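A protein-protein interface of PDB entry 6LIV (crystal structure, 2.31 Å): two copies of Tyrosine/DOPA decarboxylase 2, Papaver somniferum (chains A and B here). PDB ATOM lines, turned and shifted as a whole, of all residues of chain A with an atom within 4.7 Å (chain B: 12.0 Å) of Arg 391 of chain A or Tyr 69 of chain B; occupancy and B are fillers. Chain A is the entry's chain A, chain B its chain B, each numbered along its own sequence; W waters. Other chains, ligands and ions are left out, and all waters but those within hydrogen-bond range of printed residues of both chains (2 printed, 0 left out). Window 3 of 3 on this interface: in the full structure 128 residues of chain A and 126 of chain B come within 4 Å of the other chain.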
ATOM      1  N   ILE A 296     -16.137   1.027  19.267  1.00  0.00           N
ATOM      2  CA  ILE A 296     -15.632   2.273  18.698  1.00  0.00           C
ATOM      3  C   ILE A 296     -14.691   2.956  19.678  1.00  0.00           C
ATOM      4  O   ILE A 296     -13.890   3.810  19.282  1.00  0.00           O
ATOM      5  CB  ILE A 296     -16.766   3.240  18.302  1.00  0.00           C
ATOM      6  CG1 ILE A 296     -17.569   3.679  19.531  1.00  0.00           C
ATOM      7  CG2 ILE A 296     -17.667   2.622  17.230  1.00  0.00           C
ATOM      8  CD1 ILE A 296     -18.377   4.938  19.306  1.00  0.00           C
ATOM      9  N   CYS A 297     -14.782   2.611  20.963  1.00  0.00           N
ATOM     10  CA  CYS A 297     -13.819   3.030  21.976  1.00  0.00           C
ATOM     11  C   CYS A 297     -12.594   2.121  21.921  1.00  0.00           C
ATOM     12  O   CYS A 297     -12.741   0.893  21.973  1.00  0.00           O
ATOM     13  CB  CYS A 297     -14.454   2.987  23.366  1.00  0.00           C
ATOM     14  SG  CYS A 297     -15.986   3.975  23.513  1.00  0.00           S
ATOM     15  N   PRO A 298     -11.377   2.677  21.802  1.00  0.00           N
ATOM     16  CA  PRO A 298     -10.199   1.809  21.619  1.00  0.00           C
ATOM     17  C   PRO A 298      -9.994   0.815  22.745  1.00  0.00           C
ATOM     18  O   PRO A 298      -9.510  -0.294  22.493  1.00  0.00           O
ATOM     19  CB  PRO A 298      -9.039   2.814  21.528  1.00  0.00           C
ATOM     20  CG  PRO A 298      -9.650   4.098  21.089  1.00  0.00           C
ATOM     21  CD  PRO A 298     -11.030   4.110  21.730  1.00  0.00           C
ATOM     22  N   GLY A 386     -21.033  13.181  17.046  1.00  0.00           N
ATOM     23  CA  GLY A 386     -19.625  13.028  16.753  1.00  0.00           C
ATOM     24  C   GLY A 386     -19.003  11.850  17.484  1.00  0.00           C
ATOM     25  O   GLY A 386     -19.527  11.337  18.471  1.00  0.00           O
ATOM     26  N   VAL A 387     -17.842  11.427  16.977  1.00  0.00           N
ATOM     27  CA  VAL A 387     -17.188  10.226  17.493  1.00  0.00           C
ATOM     28  C   VAL A 387     -16.834  10.389  18.967  1.00  0.00           C
ATOM     29  O   VAL A 387     -17.031   9.470  19.771  1.00  0.00           O
ATOM     30  CB  VAL A 387     -15.946   9.892  16.645  1.00  0.00           C
ATOM     31  CG1 VAL A 387     -15.147   8.768  17.289  1.00  0.00           C
ATOM     32  CG2 VAL A 387     -16.355   9.519  15.229  1.00  0.00           C
ATOM     33  N   THR A 388     -16.316  11.560  19.346  1.00  0.00           N
ATOM     34  CA  THR A 388     -15.857  11.761  20.718  1.00  0.00           C
ATOM     35  C   THR A 388     -17.008  11.648  21.712  1.00  0.00           C
ATOM     36  O   THR A 388     -16.911  10.922  22.709  1.00  0.00           O
ATOM     37  CB  THR A 388     -15.163  13.117  20.847  1.00  0.00           C
ATOM     38  OG1 THR A 388     -14.061  13.180  19.933  1.00  0.00           O
ATOM     39  CG2 THR A 388     -14.646  13.317  22.266  1.00  0.00           C
ATOM     40  N   ASN A 389     -18.107  12.361  21.460  1.00  0.00           N
ATOM     41  CA  ASN A 389     -19.241  12.311  22.379  1.00  0.00           C
ATOM     42  C   ASN A 389     -19.897  10.937  22.381  1.00  0.00           C
ATOM     43  O   ASN A 389     -20.367  10.470  23.425  1.00  0.00           O
ATOM     44  CB  ASN A 389     -20.264  13.388  22.020  1.00  0.00           C
ATOM     45  CG  ASN A 389     -19.783  14.785  22.354  1.00  0.00           C
ATOM     46  OD1 ASN A 389     -18.846  14.962  23.132  1.00  0.00           O
ATOM     47  ND2 ASN A 389     -20.425  15.788  21.765  1.00  0.00           N
ATOM     48  N   LEU A 390     -19.945  10.277  21.220  1.00  0.00           N
ATOM     49  CA  LEU A 390     -20.532   8.942  21.158  1.00  0.00           C
ATOM     50  C   LEU A 390     -19.717   7.947  21.974  1.00  0.00           C
ATOM     51  O   LEU A 390     -20.281   7.107  22.685  1.00  0.00           O
ATOM     52  CB  LEU A 390     -20.647   8.484  19.703  1.00  0.00           C
ATOM     53  CG  LEU A 390     -21.782   9.124  18.900  1.00  0.00           C
ATOM     54  CD1 LEU A 390     -21.611   8.857  17.413  1.00  0.00           C
ATOM     55  CD2 LEU A 390     -23.133   8.629  19.390  1.00  0.00           C
ATOM     56  N   ARG A 391     -18.387   8.029  21.882  1.00  0.00           N
ATOM     57  CA  ARG A 391     -17.532   7.209  22.734  1.00  0.00           C
ATOM     58  C   ARG A 391     -17.833   7.447  24.209  1.00  0.00           C
ATOM     59  O   ARG A 391     -17.874   6.502  25.004  1.00  0.00           O
ATOM     60  CB  ARG A 391     -16.060   7.510  22.450  1.00  0.00           C
ATOM     61  CG  ARG A 391     -15.513   6.936  21.156  1.00  0.00           C
ATOM     62  CD  ARG A 391     -14.023   7.237  21.040  1.00  0.00           C
ATOM     63  NE  ARG A 391     -13.446   6.779  19.780  1.00  0.00           N
ATOM     64  CZ  ARG A 391     -12.257   7.164  19.326  1.00  0.00           C
ATOM     65  NH1 ARG A 391     -11.522   8.012  20.032  1.00  0.00           N
ATOM     66  NH2 ARG A 391     -11.802   6.704  18.169  1.00  0.00           N
ATOM     67  N   ASN A 392     -18.052   8.708  24.590  1.00  0.00           N
ATOM     68  CA  ASN A 392     -18.252   9.033  25.997  1.00  0.00           C
ATOM     69  C   ASN A 392     -19.638   8.629  26.481  1.00  0.00           C
ATOM     70  O   ASN A 392     -19.809   8.323  27.668  1.00  0.00           O
ATOM     71  CB  ASN A 392     -18.013  10.526  26.224  1.00  0.00           C
ATOM     72  CG  ASN A 392     -16.558  10.913  26.040  1.00  0.00           C
ATOM     73  OD1 ASN A 392     -15.660  10.083  26.186  1.00  0.00           O
ATOM     74  ND2 ASN A 392     -16.318  12.179  25.716  1.00  0.00           N
ATOM     75  N   PHE A 393     -20.636   8.637  25.594  1.00  0.00           N
ATOM     76  CA  PHE A 393     -21.949   8.111  25.955  1.00  0.00           C
ATOM     77  C   PHE A 393     -21.847   6.657  26.394  1.00  0.00           C
ATOM     78  O   PHE A 393     -22.343   6.278  27.462  1.00  0.00           O
ATOM     79  CB  PHE A 393     -22.911   8.238  24.775  1.00  0.00           C
ATOM     80  CG  PHE A 393     -23.259   9.651  24.409  1.00  0.00           C
ATOM     81  CD1 PHE A 393     -23.174  10.673  25.340  1.00  0.00           C
ATOM     82  CD2 PHE A 393     -23.689   9.952  23.127  1.00  0.00           C
ATOM     83  CE1 PHE A 393     -23.502  11.973  24.993  1.00  0.00           C
ATOM     84  CE2 PHE A 393     -24.017  11.245  22.775  1.00  0.00           C
ATOM     85  CZ  PHE A 393     -23.923  12.257  23.708  1.00  0.00           C
ATOM     86  N   LEU A 394     -21.200   5.825  25.571  1.00  0.00           N
ATOM     87  CA  LEU A 394     -21.033   4.417  25.910  1.00  0.00           C
ATOM     88  C   LEU A 394     -20.181   4.247  27.160  1.00  0.00           C
ATOM     89  O   LEU A 394     -20.456   3.378  27.996  1.00  0.00           O
ATOM     90  CB  LEU A 394     -20.410   3.671  24.732  1.00  0.00           C
ATOM     91  CG  LEU A 394     -21.108   3.876  23.388  1.00  0.00           C
ATOM     92  CD1 LEU A 394     -20.284   3.290  22.254  1.00  0.00           C
ATOM     93  CD2 LEU A 394     -22.494   3.261  23.422  1.00  0.00           C
ATOM     94  N   ARG A 395     -19.139   5.070  27.304  1.00  0.00           N
ATOM     95  CA  ARG A 395     -18.281   4.977  28.480  1.00  0.00           C
ATOM     96  C   ARG A 395     -19.057   5.271  29.757  1.00  0.00           C
ATOM     97  O   ARG A 395     -18.850   4.612  30.782  1.00  0.00           O
ATOM     98  CB  ARG A 395     -17.094   5.929  28.342  1.00  0.00           C
ATOM     99  CG  ARG A 395     -15.965   5.391  27.482  1.00  0.00           C
ATOM    100  CD  ARG A 395     -15.162   6.521  26.863  1.00  0.00           C
ATOM    101  NE  ARG A 395     -14.081   6.020  26.021  1.00  0.00           N
ATOM    102  CZ  ARG A 395     -13.389   6.769  25.168  1.00  0.00           C
ATOM    103  NH1 ARG A 395     -13.666   8.060  25.043  1.00  0.00           N
ATOM    104  NH2 ARG A 395     -12.422   6.228  24.442  1.00  0.00           N
ATOM    105  N   VAL B  18     -22.440  18.274  29.548  1.00  0.00           N
ATOM    106  CA  VAL B  18     -22.826  17.277  28.556  1.00  0.00           C
ATOM    107  C   VAL B  18     -24.344  17.168  28.562  1.00  0.00           C
ATOM    108  O   VAL B  18     -24.946  16.820  29.585  1.00  0.00           O
ATOM    109  CB  VAL B  18     -22.171  15.916  28.840  1.00  0.00           C
ATOM    110  CG1 VAL B  18     -22.398  14.969  27.673  1.00  0.00           C
ATOM    111  CG2 VAL B  18     -20.686  16.093  29.112  1.00  0.00           C
ATOM    112  N   THR B  19     -24.964  17.469  27.425  1.00  0.00           N
ATOM    113  CA  THR B  19     -26.414  17.418  27.294  1.00  0.00           C
ATOM    114  C   THR B  19     -26.850  16.005  26.927  1.00  0.00           C
ATOM    115  O   THR B  19     -26.265  15.379  26.037  1.00  0.00           O
ATOM    116  CB  THR B  19     -26.900  18.412  26.239  1.00  0.00           C
ATOM    117  OG1 THR B  19     -26.298  19.692  26.473  1.00  0.00           O
ATOM    118  CG2 THR B  19     -28.413  18.554  26.300  1.00  0.00           C
ATOM    119  N   PRO B  21     -28.576  13.000  25.204  1.00  0.00           N
ATOM    120  CA  PRO B  21     -29.069  12.878  23.821  1.00  0.00           C
ATOM    121  C   PRO B  21     -30.583  12.797  23.709  1.00  0.00           C
ATOM    122  O   PRO B  21     -31.105  12.922  22.596  1.00  0.00           O
ATOM    123  CB  PRO B  21     -28.412  11.583  23.320  1.00  0.00           C
ATOM    124  CG  PRO B  21     -27.260  11.349  24.242  1.00  0.00           C
ATOM    125  CD  PRO B  21     -27.675  11.896  25.572  1.00  0.00           C
ATOM    126  N   PRO B  64     -17.924  13.748   3.462  1.00  0.00           N
ATOM    127  CA  PRO B  64     -16.613  13.316   3.958  1.00  0.00           C
ATOM    128  C   PRO B  64     -16.519  11.800   4.043  1.00  0.00           C
ATOM    129  O   PRO B  64     -17.521  11.081   4.057  1.00  0.00           O
ATOM    130  CB  PRO B  64     -16.524  13.957   5.349  1.00  0.00           C
ATOM    131  CG  PRO B  64     -17.933  14.319   5.707  1.00  0.00           C
ATOM    132  CD  PRO B  64     -18.617  14.628   4.417  1.00  0.00           C
ATOM    133  N   GLU B  65     -15.277  11.318   4.103  1.00  0.00           N
ATOM    134  CA  GLU B  65     -14.996   9.888   4.115  1.00  0.00           C
ATOM    135  C   GLU B  65     -15.081   9.267   5.502  1.00  0.00           C
ATOM    136  O   GLU B  65     -15.144   8.038   5.608  1.00  0.00           O
ATOM    137  CB  GLU B  65     -13.605   9.623   3.530  1.00  0.00           C
ATOM    138  CG  GLU B  65     -13.588   9.451   2.020  1.00  0.00           C
ATOM    139  CD  GLU B  65     -12.361  10.064   1.379  1.00  0.00           C
ATOM    140  OE1 GLU B  65     -12.394  10.321   0.156  1.00  0.00           O
ATOM    141  OE2 GLU B  65     -11.364  10.291   2.096  1.00  0.00           O
ATOM    142  N   THR B  66     -15.078  10.074   6.561  1.00  0.00           N
ATOM    143  CA  THR B  66     -15.134   9.573   7.926  1.00  0.00           C
ATOM    144  C   THR B  66     -16.179  10.346   8.716  1.00  0.00           C
ATOM    145  O   THR B  66     -16.592  11.444   8.335  1.00  0.00           O
ATOM    146  CB  THR B  66     -13.772   9.682   8.630  1.00  0.00           C
ATOM    147  OG1 THR B  66     -13.340  11.048   8.629  1.00  0.00           O
ATOM    148  CG2 THR B  66     -12.731   8.823   7.930  1.00  0.00           C
ATOM    149  N   ALA B  67     -16.606   9.752   9.828  1.00  0.00           N
ATOM    150  CA  ALA B  67     -17.537  10.426  10.715  1.00  0.00           C
ATOM    151  C   ALA B  67     -16.845  11.601  11.405  1.00  0.00           C
ATOM    152  O   ALA B  67     -15.638  11.559  11.660  1.00  0.00           O
ATOM    153  CB  ALA B  67     -18.081   9.456  11.758  1.00  0.00           C
ATOM    154  N   PRO B  68     -17.583  12.666  11.711  1.00  0.00           N
ATOM    155  CA  PRO B  68     -16.964  13.804  12.397  1.00  0.00           C
ATOM    156  C   PRO B  68     -16.655  13.460  13.845  1.00  0.00           C
ATOM    157  O   PRO B  68     -17.392  12.718  14.498  1.00  0.00           O
ATOM    158  CB  PRO B  68     -18.029  14.900  12.295  1.00  0.00           C
ATOM    159  CG  PRO B  68     -19.316  14.147  12.238  1.00  0.00           C
ATOM    160  CD  PRO B  68     -19.025  12.874  11.484  1.00  0.00           C
ATOM    161  N   TYR B  69     -15.541  13.997  14.342  1.00  0.00           N
ATOM    162  CA  TYR B  69     -15.182  13.787  15.738  1.00  0.00           C
ATOM    163  C   TYR B  69     -15.933  14.718  16.676  1.00  0.00           C
ATOM    164  O   TYR B  69     -16.086  14.394  17.858  1.00  0.00           O
ATOM    165  CB  TYR B  69     -13.675  13.965  15.928  1.00  0.00           C
ATOM    166  CG  TYR B  69     -12.899  12.679  15.773  1.00  0.00           C
ATOM    167  CD1 TYR B  69     -12.451  12.261  14.527  1.00  0.00           C
ATOM    168  CD2 TYR B  69     -12.620  11.877  16.873  1.00  0.00           C
ATOM    169  CE1 TYR B  69     -11.744  11.083  14.380  1.00  0.00           C
ATOM    170  CE2 TYR B  69     -11.914  10.698  16.736  1.00  0.00           C
ATOM    171  CZ  TYR B  69     -11.479  10.306  15.487  1.00  0.00           C
ATOM    172  OH  TYR B  69     -10.775   9.133  15.345  1.00  0.00           O
ATOM    173  N   ASN B  70     -16.410  15.856  16.177  1.00  0.00           N
ATOM    174  CA  ASN B  70     -17.129  16.824  16.984  1.00  0.00           C
ATOM    175  C   ASN B  70     -18.554  16.988  16.470  1.00  0.00           C
ATOM    176  O   ASN B  70     -18.814  16.810  15.275  1.00  0.00           O
ATOM    177  CB  ASN B  70     -16.413  18.181  16.974  1.00  0.00           C
ATOM    178  CG  ASN B  70     -15.053  18.121  17.644  1.00  0.00           C
ATOM    179  OD1 ASN B  70     -14.937  17.721  18.803  1.00  0.00           O
ATOM    180  ND2 ASN B  70     -14.015  18.512  16.914  1.00  0.00           N
ATOM    181  N   PRO B  71     -19.500  17.319  17.348  1.00  0.00           N
ATOM    182  CA  PRO B  71     -20.900  17.407  16.924  1.00  0.00           C
ATOM    183  C   PRO B  71     -21.132  18.523  15.919  1.00  0.00           C
ATOM    184  O   PRO B  71     -20.477  19.568  15.944  1.00  0.00           O
ATOM    185  CB  PRO B  71     -21.651  17.682  18.234  1.00  0.00           C
ATOM    186  CG  PRO B  71     -20.623  18.254  19.152  1.00  0.00           C
ATOM    187  CD  PRO B  71     -19.345  17.563  18.792  1.00  0.00           C
ATOM    188  N   GLU B  72     -22.083  18.282  15.023  1.00  0.00           N
ATOM    189  CA  GLU B  72     -22.551  19.276  14.073  1.00  0.00           C
ATOM    190  C   GLU B  72     -23.961  19.711  14.452  1.00  0.00           C
ATOM    191  O   GLU B  72     -24.722  18.948  15.053  1.00  0.00           O
ATOM    192  CB  GLU B  72     -22.534  18.729  12.642  1.00  0.00           C
ATOM    193  CG  GLU B  72     -21.345  17.833  12.339  1.00  0.00           C
ATOM    194  CD  GLU B  72     -21.056  17.725  10.853  1.00  0.00           C
ATOM    195  OE1 GLU B  72     -20.808  18.770  10.216  1.00  0.00           O
ATOM    196  OE2 GLU B  72     -21.077  16.594  10.323  1.00  0.00           O
ATOM    197  N   SER B  73     -24.301  20.947  14.101  1.00  0.00           N
ATOM    198  CA  SER B  73     -25.602  21.490  14.463  1.00  0.00           C
ATOM    199  C   SER B  73     -26.704  20.860  13.619  1.00  0.00           C
ATOM    200  O   SER B  73     -26.486  20.445  12.477  1.00  0.00           O
ATOM    201  CB  SER B  73     -25.616  23.009  14.289  1.00  0.00           C
ATOM    202  OG  SER B  73     -25.516  23.369  12.922  1.00  0.00           O
ATOM    203  N   ILE B  77     -27.047  20.236   9.542  1.00  0.00           N
ATOM    204  CA  ILE B  77     -27.462  18.946   8.995  1.00  0.00           C
ATOM    205  C   ILE B  77     -28.672  19.118   8.086  1.00  0.00           C
ATOM    206  O   ILE B  77     -28.722  18.565   6.981  1.00  0.00           O
ATOM    207  CB  ILE B  77     -27.750  17.949  10.130  1.00  0.00           C
ATOM    208  CG1 ILE B  77     -26.465  17.610  10.885  1.00  0.00           C
ATOM    209  CG2 ILE B  77     -28.377  16.687   9.572  1.00  0.00           C
ATOM    210  CD1 ILE B  77     -26.699  16.837  12.168  1.00  0.00           C
HETATM  211  O   HOH W   1     -18.218  14.438  19.653  1.00  0.00           O
HETATM  212  O   HOH W   2     -13.090  15.398  19.205  1.00  0.00           O
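The side-chain hydroxyl of Thr 388 of chain A is in hydrogen-bond range of the backbone carbonyl oxygen of Tyr 69 of chain B, at 3.1 Å. O of Pro 68 of chain B sits at hydrogen-bond distance from N of Val 387 of chain A, 2.8 Å away.
The backbone carbonyl oxygen (O) of Thr 388 of chain A is in hydrogen-bond range of the side-chain amide nitrogen (ND2) of Asn 392 of chain A (3.3 Å). NE of Arg 391 of chain A lies within hydrogen-bond range of O of Ile 296 of chain A (3.0 Å). The backbone carbonyl oxygen (O) of Arg 391 of chain A lies within hydrogen-bond range of the side-chain sulfur (SG) of Cys 297 of chain A.
Water W2 lies within hydrogen-bond range of the side-chain hydroxyl (OG1) of Thr 388 of chain A (2.5 Å), the side-chain amide oxygen (OD1) of Asn 70 of chain B (3.0 Å) and the backbone carbonyl oxygen (O) of Tyr 69 of chain B (3.4 Å). Water W1 lies within hydrogen-bond range of the backbone NH (N) of Asn 389 of chain A (2.8 Å), the backbone carbonyl oxygen (O) of Tyr 69 of chain B (2.8 Å) and the backbone NH (N) of Thr 388 of chain A (3.5 Å).
Among the printed residues, pairs that only touch across the chains: Gly 386 of chain A with Pro 68 of chain B (3.2 Å), Gly 386 of chain A with Tyr 69 of chain B (3.9 Å), Val 387 of chain A with Ala 67 of chain B (3.9 Å), Val 387 of chain A with Tyr 69 of chain B (3.6 Å), Asn 389 of chain A with Pro 71 of chain B (3.6 Å), Arg 391 of chain A with Tyr 69 of chain B (3.9 Å) and Phe 393 of chain A with Pro 21 of chain B (3.5 Å).
No residue of chain B comes within 4 Å of Cys 297 of chain A. Gly 386 of chain A touches just these residues of chain B: Pro 68 (3.2 Å) and Tyr 69 (3.9 Å). Thr 388 of chain A touches just one residue of chain B: Tyr 69. Asn 389 of chain A touches just one residue of chain B: Pro 71 (3.6 Å). No residue of chain B comes within 4 Å of Leu 390 of chain A. Arg 391 of chain A touches just one residue of chain B: Tyr 69 (3.9 Å). Phe 393 of chain A touches just one residue of chain B: Pro 21. No residue of chain B comes within 4 Å of Leu 394 of chain A. No residue of chain B comes within 4 Å of Arg 395 of chain A. Printed residues of chain A within 4 Å of Pro 21 of chain B: Phe 393. Printed residues of chain A within 4 Å of Pro 68 of chain B: Gly 386 (3.2 Å) and Val 387 (2.8 Å). Of chain A, only Gly 386 (3.9 Å), Val 387 (3.6 Å), Thr 388 (3.1 Å) and Arg 391 (3.9 Å) come within 4 Å of Tyr 69 of chain B. Of the printed residues of chain A, Pro 71 of chain B touches Asn 389 (3.6 Å). Ser 73 of chain B touches none of the printed residues of chain A. The nearest printed residue of chain A that does not touch Pro 68 of chain B is Thr 388 of chain A (5.1 Å).
No position is printed for both chains. Of the 9 pairs that touch across the chains among the printed residues, none has its exchanged pair printed and touching as well.
Of the 13 printed residues of chain A, 6 touch a printed residue of chain B. Hydrophobic or aromatic side chains of chain A that line the printed part of chain B: Val 387 and Phe 393. Of the 14 printed residues of chain B, 5 touch a printed residue of chain A. Printed residues of chain B that touch a printed residue of chain A: Pro 21, Ala 67, Pro 68, Tyr 69 and Pro 71. Hydrophobic or aromatic side chains of chain B that line the printed part of chain A: Pro 21, Ala 67, Tyr 69 and Pro 71. Along chain B the printed residues that touch a printed residue of chain A span positions 21 to 71.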
